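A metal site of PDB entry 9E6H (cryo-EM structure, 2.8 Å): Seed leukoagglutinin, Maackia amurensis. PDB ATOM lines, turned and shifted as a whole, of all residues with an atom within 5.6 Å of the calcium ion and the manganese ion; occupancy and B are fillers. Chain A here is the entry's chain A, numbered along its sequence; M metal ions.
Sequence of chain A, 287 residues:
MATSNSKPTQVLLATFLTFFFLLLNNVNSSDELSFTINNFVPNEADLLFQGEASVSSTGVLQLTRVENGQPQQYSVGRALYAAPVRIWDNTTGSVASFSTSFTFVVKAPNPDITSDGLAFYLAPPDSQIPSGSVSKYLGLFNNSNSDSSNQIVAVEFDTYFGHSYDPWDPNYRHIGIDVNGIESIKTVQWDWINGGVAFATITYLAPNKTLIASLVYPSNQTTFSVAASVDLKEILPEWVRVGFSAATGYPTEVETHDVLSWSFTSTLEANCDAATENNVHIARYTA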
ATOM      1  N   ASP A 116     -20.006  35.094  27.454  1.00  0.00           N
ATOM      2  CA  ASP A 116     -19.600  33.786  27.960  1.00  0.00           C
ATOM      3  C   ASP A 116     -19.685  33.722  29.481  1.00  0.00           C
ATOM      4  O   ASP A 116     -20.793  33.752  30.035  1.00  0.00           O
ATOM      5  CB  ASP A 116     -18.191  33.461  27.466  1.00  0.00           C
ATOM      6  CG  ASP A 116     -18.130  33.279  25.966  1.00  0.00           C
ATOM      7  OD1 ASP A 116     -19.148  32.871  25.362  1.00  0.00           O
ATOM      8  OD2 ASP A 116     -17.064  33.557  25.372  1.00  0.00           O
ATOM      9  N   LYS A 136     -17.689  30.187  23.382  1.00  0.00           N
ATOM     10  CA  LYS A 136     -19.033  29.868  23.843  1.00  0.00           C
ATOM     11  C   LYS A 136     -19.079  28.634  24.733  1.00  0.00           C
ATOM     12  O   LYS A 136     -20.102  28.424  25.405  1.00  0.00           O
ATOM     13  CB  LYS A 136     -19.964  29.677  22.632  1.00  0.00           C
ATOM     14  CG  LYS A 136     -19.619  28.481  21.750  1.00  0.00           C
ATOM     15  CD  LYS A 136     -20.589  28.315  20.596  1.00  0.00           C
ATOM     16  CE  LYS A 136     -20.416  29.388  19.533  1.00  0.00           C
ATOM     17  NZ  LYS A 136     -19.113  29.284  18.829  1.00  0.00           N
ATOM     18  N   GLU A 156     -20.834  25.963  36.025  1.00  0.00           N
ATOM     19  CA  GLU A 156     -20.667  27.152  35.217  1.00  0.00           C
ATOM     20  C   GLU A 156     -21.587  28.266  35.695  1.00  0.00           C
ATOM     21  O   GLU A 156     -22.719  28.029  36.111  1.00  0.00           O
ATOM     22  CB  GLU A 156     -20.939  26.856  33.741  1.00  0.00           C
ATOM     23  CG  GLU A 156     -22.403  26.600  33.393  1.00  0.00           C
ATOM     24  CD  GLU A 156     -22.609  26.347  31.907  1.00  0.00           C
ATOM     25  OE1 GLU A 156     -21.604  26.176  31.186  1.00  0.00           O
ATOM     26  OE2 GLU A 156     -23.777  26.329  31.462  1.00  0.00           O
ATOM     27  N   ASP A 158     -22.998  30.986  33.749  1.00  0.00           N
ATOM     28  CA  ASP A 158     -23.156  31.447  32.380  1.00  0.00           C
ATOM     29  C   ASP A 158     -23.950  32.747  32.379  1.00  0.00           C
ATOM     30  O   ASP A 158     -25.102  32.788  32.827  1.00  0.00           O
ATOM     31  CB  ASP A 158     -23.862  30.395  31.526  1.00  0.00           C
ATOM     32  CG  ASP A 158     -23.827  30.719  30.043  1.00  0.00           C
ATOM     33  OD1 ASP A 158     -24.534  31.662  29.626  1.00  0.00           O
ATOM     34  OD2 ASP A 158     -23.108  30.031  29.290  1.00  0.00           O
ATOM     35  N   THR A 159     -23.318  33.807  31.867  1.00  0.00           N
ATOM     36  CA  THR A 159     -23.924  35.134  31.799  1.00  0.00           C
ATOM     37  C   THR A 159     -24.420  35.481  30.404  1.00  0.00           C
ATOM     38  O   THR A 159     -25.017  36.551  30.227  1.00  0.00           O
ATOM     39  CB  THR A 159     -22.913  36.194  32.250  1.00  0.00           C
ATOM     40  OG1 THR A 159     -21.787  36.196  31.371  1.00  0.00           O
ATOM     41  CG2 THR A 159     -22.433  35.898  33.667  1.00  0.00           C
ATOM     42  N   TYR A 160     -24.198  34.621  29.412  1.00  0.00           N
ATOM     43  CA  TYR A 160     -24.608  34.854  28.037  1.00  0.00           C
ATOM     44  C   TYR A 160     -25.786  33.936  27.725  1.00  0.00           C
ATOM     45  O   TYR A 160     -25.643  32.704  27.731  1.00  0.00           O
ATOM     46  CB  TYR A 160     -23.453  34.612  27.071  1.00  0.00           C
ATOM     47  CG  TYR A 160     -23.755  34.972  25.625  1.00  0.00           C
ATOM     48  CD1 TYR A 160     -24.265  36.219  25.293  1.00  0.00           C
ATOM     49  CD2 TYR A 160     -23.523  34.054  24.607  1.00  0.00           C
ATOM     50  CE1 TYR A 160     -24.540  36.541  23.980  1.00  0.00           C
ATOM     51  CE2 TYR A 160     -23.798  34.376  23.294  1.00  0.00           C
ATOM     52  CZ  TYR A 160     -24.300  35.622  22.977  1.00  0.00           C
ATOM     53  OH  TYR A 160     -24.575  35.937  21.676  1.00  0.00           O
ATOM     54  N   PHE A 161     -26.956  34.529  27.454  1.00  0.00           N
ATOM     55  CA  PHE A 161     -28.176  33.784  27.213  1.00  0.00           C
ATOM     56  C   PHE A 161     -28.564  33.775  25.737  1.00  0.00           C
ATOM     57  O   PHE A 161     -29.741  33.580  25.411  1.00  0.00           O
ATOM     58  CB  PHE A 161     -29.333  34.353  28.056  1.00  0.00           C
ATOM     59  CG  PHE A 161     -29.317  35.849  28.196  1.00  0.00           C
ATOM     60  CD1 PHE A 161     -29.924  36.654  27.244  1.00  0.00           C
ATOM     61  CD2 PHE A 161     -28.686  36.447  29.273  1.00  0.00           C
ATOM     62  CE1 PHE A 161     -29.907  38.030  27.378  1.00  0.00           C
ATOM     63  CE2 PHE A 161     -28.674  37.830  29.404  1.00  0.00           C
ATOM     64  CZ  PHE A 161     -29.283  38.622  28.452  1.00  0.00           C
ATOM     65  N   GLY A 162     -27.609  33.989  24.841  1.00  0.00           N
ATOM     66  CA  GLY A 162     -27.922  34.037  23.428  1.00  0.00           C
ATOM     67  C   GLY A 162     -28.521  32.730  22.936  1.00  0.00           C
ATOM     68  O   GLY A 162     -28.187  31.647  23.412  1.00  0.00           O
ATOM     69  N   ASP A 166     -25.840  30.074  21.478  1.00  0.00           N
ATOM     70  CA  ASP A 166     -25.996  29.141  22.589  1.00  0.00           C
ATOM     71  C   ASP A 166     -27.439  28.672  22.632  1.00  0.00           C
ATOM     72  O   ASP A 166     -28.187  29.015  23.571  1.00  0.00           O
ATOM     73  CB  ASP A 166     -25.593  29.774  23.926  1.00  0.00           C
ATOM     74  CG  ASP A 166     -24.109  30.091  24.006  1.00  0.00           C
ATOM     75  OD1 ASP A 166     -23.400  29.935  22.989  1.00  0.00           O
ATOM     76  OD2 ASP A 166     -23.655  30.498  25.095  1.00  0.00           O
ATOM     77  N   TRP A 168     -28.533  25.793  23.380  1.00  0.00           N
ATOM     78  CA  TRP A 168     -28.735  24.907  24.520  1.00  0.00           C
ATOM     79  C   TRP A 168     -29.030  25.675  25.798  1.00  0.00           C
ATOM     80  O   TRP A 168     -29.827  25.213  26.624  1.00  0.00           O
ATOM     81  CB  TRP A 168     -27.510  24.004  24.723  1.00  0.00           C
ATOM     82  CG  TRP A 168     -26.212  24.756  24.858  1.00  0.00           C
ATOM     83  CD1 TRP A 168     -25.670  25.262  25.993  1.00  0.00           C
ATOM     84  CD2 TRP A 168     -25.304  25.080  23.792  1.00  0.00           C
ATOM     85  NE1 TRP A 168     -24.475  25.879  25.720  1.00  0.00           N
ATOM     86  CE2 TRP A 168     -24.218  25.780  24.374  1.00  0.00           C
ATOM     87  CE3 TRP A 168     -25.288  24.846  22.419  1.00  0.00           C
ATOM     88  CZ2 TRP A 168     -23.151  26.249  23.621  1.00  0.00           C
ATOM     89  CZ3 TRP A 168     -24.221  25.307  21.678  1.00  0.00           C
ATOM     90  CH2 TRP A 168     -23.168  26.003  22.276  1.00  0.00           C
ATOM     91  N   ASP A 169     -28.397  26.830  25.995  1.00  0.00           N
ATOM     92  CA  ASP A 169     -28.576  27.581  27.225  1.00  0.00           C
ATOM     93  C   ASP A 169     -29.993  28.146  27.311  1.00  0.00           C
ATOM     94  O   ASP A 169     -30.618  28.420  26.273  1.00  0.00           O
ATOM     95  CB  ASP A 169     -27.565  28.711  27.316  1.00  0.00           C
ATOM     96  CG  ASP A 169     -26.221  28.261  27.874  1.00  0.00           C
ATOM     97  OD1 ASP A 169     -26.184  27.268  28.638  1.00  0.00           O
ATOM     98  OD2 ASP A 169     -25.199  28.899  27.548  1.00  0.00           O
ATOM     99  N   PRO A 170     -30.535  28.331  28.524  1.00  0.00           N
ATOM    100  CA  PRO A 170     -31.863  28.952  28.646  1.00  0.00           C
ATOM    101  C   PRO A 170     -31.868  30.434  28.279  1.00  0.00           C
ATOM    102  O   PRO A 170     -30.835  30.992  27.882  1.00  0.00           O
ATOM    103  CB  PRO A 170     -32.203  28.746  30.122  1.00  0.00           C
ATOM    104  CG  PRO A 170     -30.898  28.591  30.804  1.00  0.00           C
ATOM    105  CD  PRO A 170     -30.029  27.869  29.827  1.00  0.00           C
ATOM    106  N   HIS A 174     -27.724  32.181  34.050  1.00  0.00           N
ATOM    107  CA  HIS A 174     -27.964  30.977  34.827  1.00  0.00           C
ATOM    108  C   HIS A 174     -26.684  30.448  35.457  1.00  0.00           C
ATOM    109  O   HIS A 174     -25.574  30.815  35.068  1.00  0.00           O
ATOM    110  CB  HIS A 174     -28.605  29.884  33.954  1.00  0.00           C
ATOM    111  CG  HIS A 174     -27.884  29.627  32.674  1.00  0.00           C
ATOM    112  ND1 HIS A 174     -27.951  30.479  31.601  1.00  0.00           N
ATOM    113  CD2 HIS A 174     -27.100  28.595  32.275  1.00  0.00           C
ATOM    114  CE1 HIS A 174     -27.221  30.002  30.602  1.00  0.00           C
ATOM    115  NE2 HIS A 174     -26.702  28.854  30.990  1.00  0.00           N
ATOM    116  N   ILE A 182     -21.405  20.728  27.296  1.00  0.00           N
ATOM    117  CA  ILE A 182     -21.809  22.097  27.594  1.00  0.00           C
ATOM    118  C   ILE A 182     -23.268  22.163  28.039  1.00  0.00           C
ATOM    119  O   ILE A 182     -23.612  22.997  28.883  1.00  0.00           O
ATOM    120  CB  ILE A 182     -21.567  23.001  26.372  1.00  0.00           C
ATOM    121  CG1 ILE A 182     -21.687  24.481  26.746  1.00  0.00           C
ATOM    122  CG2 ILE A 182     -22.536  22.665  25.251  1.00  0.00           C
ATOM    123  CD1 ILE A 182     -20.611  24.964  27.702  1.00  0.00           C
ATOM    124  N   SER A 184     -25.986  21.831  30.195  1.00  0.00           N
ATOM    125  CA  SER A 184     -26.051  21.551  31.623  1.00  0.00           C
ATOM    126  C   SER A 184     -27.250  20.680  31.954  1.00  0.00           C
ATOM    127  O   SER A 184     -28.360  20.912  31.471  1.00  0.00           O
ATOM    128  CB  SER A 184     -26.133  22.867  32.407  1.00  0.00           C
ATOM    129  OG  SER A 184     -24.957  23.635  32.231  1.00  0.00           O
ATOM    130  N   THR A 187     -29.935  23.658  35.685  1.00  0.00           N
ATOM    131  CA  THR A 187     -29.613  25.087  35.737  1.00  0.00           C
ATOM    132  C   THR A 187     -30.600  25.797  36.647  1.00  0.00           C
ATOM    133  O   THR A 187     -31.731  25.359  36.832  1.00  0.00           O
ATOM    134  CB  THR A 187     -29.649  25.715  34.336  1.00  0.00           C
ATOM    135  OG1 THR A 187     -30.957  25.551  33.772  1.00  0.00           O
ATOM    136  CG2 THR A 187     -28.627  25.073  33.431  1.00  0.00           C
HETATM  137 CA    CA M   1     -24.143  31.003  27.384  1.00  0.00          CA
HETATM  138 MN    MN M   2     -24.924  27.732  30.310  1.00  0.00          MN
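Within 4 Å of the manganese ion: Glu 156, Asp 158, Asp 169 and His 174.
The manganese ion is bound by OD1 of Asp 169 (2.1 Å), OE2 of Glu 156 (2.1 Å) and NE2 of His 174 (2.2 Å).
The backbone NH (N) of Asp 158 is in hydrogen-bond range of the backbone carbonyl oxygen (O) of His 174, at 2.9 Å. The side-chain carboxylate (OE2) of Glu 156 lies close to the side-chain hydroxyl (OG) of Ser 184.
The calcium ion is bound by the backbone carbonyl oxygen (O) of Tyr 160 (2.3 Å), the side-chain carboxylate (OD2) of Asp 169 (2.4 Å), the side-chain carboxylate (OD1) of Asp 158 (2.4 Å), the side-chain carboxylate (OD2) of Asp 158 (2.4 Å) and the side-chain carboxylate (OD2) of Asp 166 (2.4 Å). The calcium ion has five donor atoms within binding distance.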
